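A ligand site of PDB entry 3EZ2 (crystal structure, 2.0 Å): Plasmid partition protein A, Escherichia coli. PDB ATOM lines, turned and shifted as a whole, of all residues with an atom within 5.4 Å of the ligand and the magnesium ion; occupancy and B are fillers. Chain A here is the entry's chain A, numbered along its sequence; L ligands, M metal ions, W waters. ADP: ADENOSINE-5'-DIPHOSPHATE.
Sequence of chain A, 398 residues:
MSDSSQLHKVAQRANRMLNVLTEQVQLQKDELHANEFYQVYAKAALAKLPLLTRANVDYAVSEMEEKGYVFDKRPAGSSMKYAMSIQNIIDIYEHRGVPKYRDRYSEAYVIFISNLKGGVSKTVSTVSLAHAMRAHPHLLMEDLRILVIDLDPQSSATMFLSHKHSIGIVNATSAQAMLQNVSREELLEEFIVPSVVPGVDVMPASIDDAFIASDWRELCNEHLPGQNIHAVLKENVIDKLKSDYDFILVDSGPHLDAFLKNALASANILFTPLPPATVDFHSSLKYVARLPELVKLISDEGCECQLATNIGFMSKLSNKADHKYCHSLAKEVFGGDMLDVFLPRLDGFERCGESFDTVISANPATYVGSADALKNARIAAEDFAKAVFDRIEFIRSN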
ATOM      1  N   LYS A 117      -1.871 -12.955   5.875  1.00  0.00           N
ATOM      2  CA  LYS A 117      -1.590 -14.130   6.692  1.00  0.00           C
ATOM      3  C   LYS A 117      -2.897 -14.894   6.822  1.00  0.00           C
ATOM      4  O   LYS A 117      -3.898 -14.326   7.265  1.00  0.00           O
ATOM      5  CB  LYS A 117      -1.092 -13.713   8.081  1.00  0.00           C
ATOM      6  CG  LYS A 117      -0.736 -14.889   8.974  1.00  0.00           C
ATOM      7  CD  LYS A 117       0.418 -15.720   8.369  1.00  0.00           C
ATOM      8  CE  LYS A 117       0.637 -17.023   9.121  1.00  0.00           C
ATOM      9  NZ  LYS A 117       1.518 -17.950   8.303  1.00  0.00           N
ATOM     10  N   GLY A 118      -2.877 -16.182   6.468  1.00  0.00           N
ATOM     11  CA  GLY A 118      -4.050 -17.011   6.546  1.00  0.00           C
ATOM     12  C   GLY A 118      -4.290 -17.635   7.898  1.00  0.00           C
ATOM     13  O   GLY A 118      -3.383 -17.650   8.727  1.00  0.00           O
ATOM     14  N   GLY A 119      -5.503 -18.135   8.118  1.00  0.00           N
ATOM     15  CA  GLY A 119      -5.856 -18.777   9.390  1.00  0.00           C
ATOM     16  C   GLY A 119      -5.906 -17.830  10.587  1.00  0.00           C
ATOM     17  O   GLY A 119      -5.852 -18.263  11.737  1.00  0.00           O
ATOM     18  N   VAL A 120      -5.991 -16.531  10.324  1.00  0.00           N
ATOM     19  CA  VAL A 120      -6.047 -15.563  11.416  1.00  0.00           C
ATOM     20  C   VAL A 120      -7.485 -15.189  11.772  1.00  0.00           C
ATOM     21  O   VAL A 120      -7.690 -14.321  12.589  1.00  0.00           O
ATOM     22  CB  VAL A 120      -5.312 -14.277  11.046  1.00  0.00           C
ATOM     23  CG1 VAL A 120      -3.828 -14.613  10.704  1.00  0.00           C
ATOM     24  CG2 VAL A 120      -6.000 -13.598   9.866  1.00  0.00           C
ATOM     25  N   SER A 121      -8.474 -15.849  11.147  1.00  0.00           N
ATOM     26  CA  SER A 121      -9.883 -15.590  11.414  1.00  0.00           C
ATOM     27  C   SER A 121     -10.584 -14.561  10.508  1.00  0.00           C
ATOM     28  O   SER A 121     -11.601 -13.980  10.897  1.00  0.00           O
ATOM     29  CB  SER A 121     -10.085 -15.168  12.880  1.00  0.00           C
ATOM     30  OG  SER A 121     -11.397 -15.460  13.293  1.00  0.00           O
ATOM     31  N   LYS A 122     -10.076 -14.329   9.307  1.00  0.00           N
ATOM     32  CA  LYS A 122     -10.764 -13.399   8.406  1.00  0.00           C
ATOM     33  C   LYS A 122     -12.197 -13.913   8.175  1.00  0.00           C
ATOM     34  O   LYS A 122     -13.147 -13.163   8.370  1.00  0.00           O
ATOM     35  CB  LYS A 122     -10.051 -13.283   7.060  1.00  0.00           C
ATOM     36  CG  LYS A 122      -8.687 -12.578   7.137  1.00  0.00           C
ATOM     37  CD  LYS A 122      -8.059 -12.358   5.734  1.00  0.00           C
ATOM     38  CE  LYS A 122      -7.674 -13.679   5.068  1.00  0.00           C
ATOM     39  NZ  LYS A 122      -6.923 -14.553   5.987  1.00  0.00           N
ATOM     40  N   THR A 123     -12.360 -15.188   7.817  1.00  0.00           N
ATOM     41  CA  THR A 123     -13.694 -15.753   7.547  1.00  0.00           C
ATOM     42  C   THR A 123     -14.645 -15.834   8.759  1.00  0.00           C
ATOM     43  O   THR A 123     -15.804 -15.380   8.699  1.00  0.00           O
ATOM     44  CB  THR A 123     -13.589 -17.163   6.870  1.00  0.00           C
ATOM     45  OG1 THR A 123     -12.939 -17.019   5.613  1.00  0.00           O
ATOM     46  CG2 THR A 123     -14.976 -17.763   6.575  1.00  0.00           C
ATOM     47  N   VAL A 124     -14.157 -16.386   9.855  1.00  0.00           N
ATOM     48  CA  VAL A 124     -14.974 -16.501  11.048  1.00  0.00           C
ATOM     49  C   VAL A 124     -15.363 -15.126  11.586  1.00  0.00           C
ATOM     50  O   VAL A 124     -16.529 -14.906  11.998  1.00  0.00           O
ATOM     51  CB  VAL A 124     -14.249 -17.266  12.168  1.00  0.00           C
ATOM     52  CG1 VAL A 124     -15.078 -17.268  13.441  1.00  0.00           C
ATOM     53  CG2 VAL A 124     -13.940 -18.693  11.728  1.00  0.00           C
ATOM     54  N   SER A 125     -14.433 -14.181  11.581  1.00  0.00           N
ATOM     55  CA  SER A 125     -14.799 -12.873  12.095  1.00  0.00           C
ATOM     56  C   SER A 125     -15.801 -12.253  11.109  1.00  0.00           C
ATOM     57  O   SER A 125     -16.780 -11.621  11.536  1.00  0.00           O
ATOM     58  CB  SER A 125     -13.530 -12.007  12.381  1.00  0.00           C
ATOM     59  OG  SER A 125     -12.963 -11.487  11.220  1.00  0.00           O
ATOM     60  N   ASP A 152     -13.517 -16.289  -2.168  1.00  0.00           N
ATOM     61  CA  ASP A 152     -12.459 -17.286  -1.992  1.00  0.00           C
ATOM     62  C   ASP A 152     -12.930 -18.583  -2.645  1.00  0.00           C
ATOM     63  O   ASP A 152     -13.941 -19.153  -2.219  1.00  0.00           O
ATOM     64  CB  ASP A 152     -12.176 -17.564  -0.492  1.00  0.00           C
ATOM     65  CG  ASP A 152     -10.998 -18.558  -0.285  1.00  0.00           C
ATOM     66  OD1 ASP A 152     -10.476 -19.137  -1.262  1.00  0.00           O
ATOM     67  OD2 ASP A 152     -10.584 -18.745   0.883  1.00  0.00           O
ATOM     68  N   SER A 156     -15.112 -20.848   2.039  1.00  0.00           N
ATOM     69  CA  SER A 156     -15.360 -21.049   3.464  1.00  0.00           C
ATOM     70  C   SER A 156     -16.516 -20.181   3.951  1.00  0.00           C
ATOM     71  O   SER A 156     -17.304 -20.654   4.728  1.00  0.00           O
ATOM     72  CB  SER A 156     -14.101 -20.736   4.275  1.00  0.00           C
ATOM     73  OG  SER A 156     -12.983 -21.419   3.716  1.00  0.00           O
ATOM     74  N   PHE A 160     -20.170 -21.581   5.677  1.00  0.00           N
ATOM     75  CA  PHE A 160     -20.626 -21.141   7.005  1.00  0.00           C
ATOM     76  C   PHE A 160     -22.035 -20.531   6.886  1.00  0.00           C
ATOM     77  O   PHE A 160     -22.909 -20.785   7.706  1.00  0.00           O
ATOM     78  CB  PHE A 160     -19.714 -20.048   7.616  1.00  0.00           C
ATOM     79  CG  PHE A 160     -18.607 -20.561   8.492  1.00  0.00           C
ATOM     80  CD1 PHE A 160     -17.305 -20.608   8.016  1.00  0.00           C
ATOM     81  CD2 PHE A 160     -18.862 -20.986   9.789  1.00  0.00           C
ATOM     82  CE1 PHE A 160     -16.258 -21.093   8.816  1.00  0.00           C
ATOM     83  CE2 PHE A 160     -17.829 -21.463  10.606  1.00  0.00           C
ATOM     84  CZ  PHE A 160     -16.531 -21.516  10.122  1.00  0.00           C
ATOM     85  N   ASP A 251     -15.201 -11.276   1.539  1.00  0.00           N
ATOM     86  CA  ASP A 251     -14.220 -12.212   2.114  1.00  0.00           C
ATOM     87  C   ASP A 251     -13.504 -12.889   0.947  1.00  0.00           C
ATOM     88  O   ASP A 251     -14.159 -13.411   0.036  1.00  0.00           O
ATOM     89  CB  ASP A 251     -14.939 -13.257   2.989  1.00  0.00           C
ATOM     90  CG  ASP A 251     -13.989 -14.160   3.818  1.00  0.00           C
ATOM     91  OD1 ASP A 251     -12.886 -13.723   4.197  1.00  0.00           O
ATOM     92  OD2 ASP A 251     -14.374 -15.327   4.108  1.00  0.00           O
ATOM     93  N   SER A 252     -12.179 -12.833   0.915  1.00  0.00           N
ATOM     94  CA  SER A 252     -11.443 -13.527  -0.146  1.00  0.00           C
ATOM     95  C   SER A 252     -10.369 -14.437   0.489  1.00  0.00           C
ATOM     96  O   SER A 252     -10.253 -14.506   1.709  1.00  0.00           O
ATOM     97  CB  SER A 252     -10.763 -12.536  -1.083  1.00  0.00           C
ATOM     98  OG  SER A 252      -9.717 -11.875  -0.414  1.00  0.00           O
ATOM     99  N   SER A 315      -7.127 -11.336  17.415  1.00  0.00           N
ATOM    100  CA  SER A 315      -8.037 -12.420  17.107  1.00  0.00           C
ATOM    101  C   SER A 315      -7.452 -13.734  17.585  1.00  0.00           C
ATOM    102  O   SER A 315      -6.274 -14.009  17.338  1.00  0.00           O
ATOM    103  CB  SER A 315      -8.248 -12.457  15.584  1.00  0.00           C
ATOM    104  OG  SER A 315      -9.230 -13.413  15.236  1.00  0.00           O
ATOM    105  N   LYS A 316      -8.274 -14.531  18.250  1.00  0.00           N
ATOM    106  CA  LYS A 316      -7.865 -15.833  18.802  1.00  0.00           C
ATOM    107  C   LYS A 316      -6.909 -15.586  19.980  1.00  0.00           C
ATOM    108  O   LYS A 316      -5.994 -16.372  20.265  1.00  0.00           O
ATOM    109  CB  LYS A 316      -7.219 -16.695  17.720  1.00  0.00           C
ATOM    110  CG  LYS A 316      -8.193 -17.032  16.573  1.00  0.00           C
ATOM    111  CD  LYS A 316      -7.542 -17.728  15.351  1.00  0.00           C
ATOM    112  CE  LYS A 316      -7.181 -19.168  15.632  1.00  0.00           C
ATOM    113  NZ  LYS A 316      -6.977 -19.933  14.339  1.00  0.00           N
ATOM    114  N   LEU A 343     -11.338 -10.620  19.869  1.00  0.00           N
ATOM    115  CA  LEU A 343     -12.044 -11.877  19.686  1.00  0.00           C
ATOM    116  C   LEU A 343     -11.205 -12.940  20.367  1.00  0.00           C
ATOM    117  O   LEU A 343     -10.145 -13.314  19.879  1.00  0.00           O
ATOM    118  CB  LEU A 343     -12.171 -12.144  18.184  1.00  0.00           C
ATOM    119  CG  LEU A 343     -13.322 -12.984  17.619  1.00  0.00           C
ATOM    120  CD1 LEU A 343     -14.691 -12.513  18.124  1.00  0.00           C
ATOM    121  CD2 LEU A 343     -13.258 -12.865  16.104  1.00  0.00           C
ATOM    122  N   PRO A 344     -11.653 -13.438  21.533  1.00  0.00           N
ATOM    123  CA  PRO A 344     -10.920 -14.468  22.284  1.00  0.00           C
ATOM    124  C   PRO A 344     -10.905 -15.809  21.590  1.00  0.00           C
ATOM    125  O   PRO A 344     -11.790 -16.119  20.775  1.00  0.00           O
ATOM    126  CB  PRO A 344     -11.677 -14.539  23.599  1.00  0.00           C
ATOM    127  CG  PRO A 344     -13.114 -14.261  23.166  1.00  0.00           C
ATOM    128  CD  PRO A 344     -12.949 -13.134  22.173  1.00  0.00           C
ATOM    129  N   ARG A 345      -9.898 -16.622  21.903  1.00  0.00           N
ATOM    130  CA  ARG A 345      -9.853 -17.960  21.351  1.00  0.00           C
ATOM    131  C   ARG A 345     -10.809 -18.677  22.302  1.00  0.00           C
ATOM    132  O   ARG A 345     -10.637 -18.543  23.514  1.00  0.00           O
ATOM    133  CB  ARG A 345      -8.445 -18.550  21.484  1.00  0.00           C
ATOM    134  CG  ARG A 345      -8.443 -20.010  21.161  1.00  0.00           C
ATOM    135  CD  ARG A 345      -7.062 -20.630  21.250  1.00  0.00           C
ATOM    136  NE  ARG A 345      -7.102 -21.886  20.519  1.00  0.00           N
ATOM    137  CZ  ARG A 345      -6.849 -22.006  19.224  1.00  0.00           C
ATOM    138  NH1 ARG A 345      -6.525 -20.943  18.500  1.00  0.00           N
ATOM    139  NH2 ARG A 345      -6.977 -23.178  18.627  1.00  0.00           N
ATOM    140  N   LEU A 346     -11.829 -19.378  21.779  1.00  0.00           N
ATOM    141  CA  LEU A 346     -12.808 -20.080  22.639  1.00  0.00           C
ATOM    142  C   LEU A 346     -13.237 -21.414  22.053  1.00  0.00           C
ATOM    143  O   LEU A 346     -13.281 -21.567  20.829  1.00  0.00           O
ATOM    144  CB  LEU A 346     -14.081 -19.218  22.864  1.00  0.00           C
ATOM    145  CG  LEU A 346     -13.971 -17.978  23.752  1.00  0.00           C
ATOM    146  CD1 LEU A 346     -15.302 -17.211  23.764  1.00  0.00           C
ATOM    147  CD2 LEU A 346     -13.562 -18.400  25.203  1.00  0.00           C
ATOM    148  N   PHE A 349     -16.158 -21.295  19.341  1.00  0.00           N
ATOM    149  CA  PHE A 349     -15.797 -20.975  17.969  1.00  0.00           C
ATOM    150  C   PHE A 349     -15.198 -22.196  17.293  1.00  0.00           C
ATOM    151  O   PHE A 349     -15.497 -22.492  16.119  1.00  0.00           O
ATOM    152  CB  PHE A 349     -14.773 -19.829  17.921  1.00  0.00           C
ATOM    153  CG  PHE A 349     -15.362 -18.474  18.217  1.00  0.00           C
ATOM    154  CD1 PHE A 349     -14.868 -17.688  19.252  1.00  0.00           C
ATOM    155  CD2 PHE A 349     -16.440 -17.991  17.464  1.00  0.00           C
ATOM    156  CE1 PHE A 349     -15.441 -16.439  19.541  1.00  0.00           C
ATOM    157  CE2 PHE A 349     -17.018 -16.746  17.745  1.00  0.00           C
ATOM    158  CZ  PHE A 349     -16.527 -15.974  18.779  1.00  0.00           C
ATOM    159  N   GLU A 350     -14.343 -22.903  18.023  1.00  0.00           N
ATOM    160  CA  GLU A 350     -13.704 -24.099  17.481  1.00  0.00           C
ATOM    161  C   GLU A 350     -14.721 -25.154  17.072  1.00  0.00           C
ATOM    162  O   GLU A 350     -14.721 -25.607  15.940  1.00  0.00           O
ATOM    163  CB  GLU A 350     -12.705 -24.690  18.477  1.00  0.00           C
ATOM    164  CG  GLU A 350     -11.311 -24.122  18.343  1.00  0.00           C
ATOM    165  CD  GLU A 350     -10.313 -24.758  19.302  1.00  0.00           C
ATOM    166  OE1 GLU A 350     -10.112 -25.993  19.233  1.00  0.00           O
ATOM    167  OE2 GLU A 350      -9.740 -23.996  20.128  1.00  0.00           O
ATOM    168  N   GLY A 353     -16.979 -24.043  14.313  1.00  0.00           N
ATOM    169  CA  GLY A 353     -16.192 -23.990  13.100  1.00  0.00           C
ATOM    170  C   GLY A 353     -16.133 -25.346  12.429  1.00  0.00           C
ATOM    171  O   GLY A 353     -16.197 -25.449  11.198  1.00  0.00           O
ATOM    172  N   GLU A 354     -16.020 -26.400  13.242  1.00  0.00           N
ATOM    173  CA  GLU A 354     -15.947 -27.759  12.727  1.00  0.00           C
ATOM    174  C   GLU A 354     -17.160 -28.117  11.863  1.00  0.00           C
ATOM    175  O   GLU A 354     -16.988 -28.655  10.776  1.00  0.00           O
ATOM    176  CB  GLU A 354     -15.801 -28.761  13.890  1.00  0.00           C
ATOM    177  CG  GLU A 354     -14.365 -28.873  14.430  1.00  0.00           C
ATOM    178  CD  GLU A 354     -14.301 -29.515  15.822  1.00  0.00           C
ATOM    179  OE1 GLU A 354     -15.242 -30.259  16.186  1.00  0.00           O
ATOM    180  OE2 GLU A 354     -13.299 -29.280  16.533  1.00  0.00           O
HETATM  181  PB  ADP L   1      -8.901 -17.090   7.519  1.00  0.00           P
HETATM  182  O1B ADP L   1      -7.919 -16.421   8.344  1.00  0.00           O
HETATM  183  O2B ADP L   1     -10.276 -16.880   7.133  1.00  0.00           O
HETATM  184  O3B ADP L   1      -8.182 -18.349   6.821  1.00  0.00           O
HETATM  185  PA  ADP L   1     -10.565 -18.839   9.343  1.00  0.00           P
HETATM  186  O1A ADP L   1     -11.678 -17.867   9.733  1.00  0.00           O
HETATM  187  O2A ADP L   1     -10.873 -19.859   8.349  1.00  0.00           O
HETATM  188  O3A ADP L   1      -9.316 -17.878   8.818  1.00  0.00           O
HETATM  189  O5' ADP L   1     -10.055 -19.342  10.745  1.00  0.00           O
HETATM  190  C5' ADP L   1      -8.983 -20.346  10.863  1.00  0.00           C
HETATM  191  C4' ADP L   1      -9.413 -21.558  11.766  1.00  0.00           C
HETATM  192  O4' ADP L   1      -9.509 -21.077  13.140  1.00  0.00           O
HETATM  193  C3' ADP L   1     -10.827 -22.237  11.526  1.00  0.00           C
HETATM  194  O3' ADP L   1     -10.691 -23.673  11.511  1.00  0.00           O
HETATM  195  C2' ADP L   1     -11.689 -21.674  12.617  1.00  0.00           C
HETATM  196  O2' ADP L   1     -12.719 -22.583  13.025  1.00  0.00           O
HETATM  197  C1' ADP L   1     -10.789 -21.310  13.792  1.00  0.00           C
HETATM  198  N9  ADP L   1     -11.055 -20.005  14.558  1.00  0.00           N
HETATM  199  C8  ADP L   1     -11.241 -18.713  14.105  1.00  0.00           C
HETATM  200  N7  ADP L   1     -11.440 -17.827  15.015  1.00  0.00           N
HETATM  201  C5  ADP L   1     -11.371 -18.561  16.182  1.00  0.00           C
HETATM  202  C6  ADP L   1     -11.504 -18.200  17.579  1.00  0.00           C
HETATM  203  N6  ADP L   1     -11.724 -16.928  17.946  1.00  0.00           N
HETATM  204  N1  ADP L   1     -11.375 -19.193  18.558  1.00  0.00           N
HETATM  205  C2  ADP L   1     -11.149 -20.511  18.191  1.00  0.00           C
HETATM  206  N3  ADP L   1     -11.012 -20.979  16.890  1.00  0.00           N
HETATM  207  C4  ADP L   1     -11.138 -19.931  15.927  1.00  0.00           C
HETATM  208 MG    MG M   1     -10.841 -17.516   4.985  1.00  0.00          MG
HETATM  209  O   HOH W   1     -13.035 -21.817   8.022  1.00  0.00           O
HETATM  210  O   HOH W   2     -15.311 -20.984  14.127  1.00  0.00           O
HETATM  211  O   HOH W   3      -9.383 -23.122  16.491  1.00  0.00           O
HETATM  212  O   HOH W   4      -8.902 -17.846   4.167  1.00  0.00           O
HETATM  213  O   HOH W   5     -10.912 -15.452   4.282  1.00  0.00           O
HETATM  214  O   HOH W   6     -11.027 -14.877  16.247  1.00  0.00           O
HETATM  215  O   HOH W   7      -6.745 -22.346   9.260  1.00  0.00           O
HETATM  216  O   HOH W   8     -11.169 -19.525   5.803  1.00  0.00           O
HETATM  217  O   HOH W   9     -12.908 -24.801  14.006  1.00  0.00           O
HETATM  218  O   HOH W  10     -11.830 -18.102   3.012  1.00  0.00           O
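N of Val 124 lies within hydrogen-bond range of O1A of the ligand, 2.9 Å away.
A nitrogen (N6) of the ligand is in hydrogen-bond range of the backbone carbonyl oxygen (O) of Pro 344 (2.9 Å).
An oxygen (O1B) of the ligand sits at hydrogen-bond distance from the backbone NH of Gly 119 (3.0 Å).
N1 of the ligand sits at hydrogen-bond distance from N of Leu 346, at 3.3 Å.
An oxygen (O1A) of the ligand lies within hydrogen-bond range of the backbone NH (N) of Thr 123.
The backbone NH (N) of Lys 122 sits at hydrogen-bond distance from an oxygen (O1B) of the ligand (3.2 Å).
An oxygen (O4') of the ligand is in hydrogen-bond range of the side-chain amino group of Lys 316 (3.0 Å).
The backbone NH of Ser 121 is in hydrogen-bond range of an oxygen (O1B) of the ligand (2.9 Å).
O1B of the ligand lies within salt-bridge range of NZ of Lys 122 (3.2 Å).
The backbone NH (N) of Val 120 sits at hydrogen-bond distance from an oxygen (O1B) of the ligand (2.8 Å).
A nitrogen (N7) of the ligand lies within hydrogen-bond range of the side-chain hydroxyl (OG) of Ser 121 (2.9 Å).
Within 4 Å of the magnesium ion: Thr 123.
The nearest printed residue that does not touch the magnesium ion is Asp 251 (4.2 Å).
Merely in contact with the ligand: Gly 118 (3.9 Å), Arg 345 (3.4 Å), Phe 349 (3.5 Å), Glu 350 (3.5 Å) and Gly 353 (3.7 Å).
Hydrophobic or aromatic side chains that line the ligand: Val 120, Val 124 and Phe 349.
Water W8 lies within hydrogen-bond range of an oxygen (O2A) of the ligand (2.6 Å) and the side-chain hydroxyl of Ser 156 (3.4 Å).
Water W5 bridges OD1 of Asp 251 (2.6 Å) and O of Ser 252 (2.8 Å).
Water W9 lies within hydrogen-bond range of an oxygen (O2') of the ligand (2.4 Å) and the backbone carbonyl oxygen (O) of Glu 350 (2.8 Å).
Water W3 lies within hydrogen-bond range of a nitrogen (N3) of the ligand (2.7 Å) and the guanidinium group (NH2) of Arg 345 (3.2 Å).
Water W6 lies within hydrogen-bond range of OG of Ser 315 (2.5 Å), N6 of the ligand (2.8 Å), OG of Ser 121 (3.0 Å) and N of Lys 316 (3.4 Å).
Water W2 lies within hydrogen-bond range of the backbone carbonyl oxygen of Phe 349, an oxygen (O2') of the ligand and the backbone NH of Gly 353.
The backbone carbonyl oxygen of Lys 122 sits at hydrogen-bond distance from the side-chain hydroxyl of Ser 125, 3.3 Å away.
The backbone carbonyl oxygen (O) of Ser 121 lies within hydrogen-bond range of the side-chain hydroxyl (OG) of Ser 125, 2.9 Å away.
The backbone carbonyl oxygen of Leu 343 is in hydrogen-bond range of the backbone NH of Lys 316 (2.8 Å).
OD2 of Asp 251 sits close to OG1 of Thr 123, 2.7 Å away.
The backbone carbonyl oxygen (O) of Lys 117 is in hydrogen-bond range of the side-chain amino group (NZ) of Lys 122 (3.3 Å).
NH2 of Arg 345 is in salt-bridge range of OE2 of Glu 350 (3.2 Å).
O of Gly 119 is in hydrogen-bond range of NZ of Lys 316 (3.3 Å).
O of Val 120 sits at hydrogen-bond distance from OG of Ser 315 (3.2 Å).
The magnesium ion is bound by water W4, water W5, water W8, OG1 of Thr 123, water W10 and O2B of the ligand.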
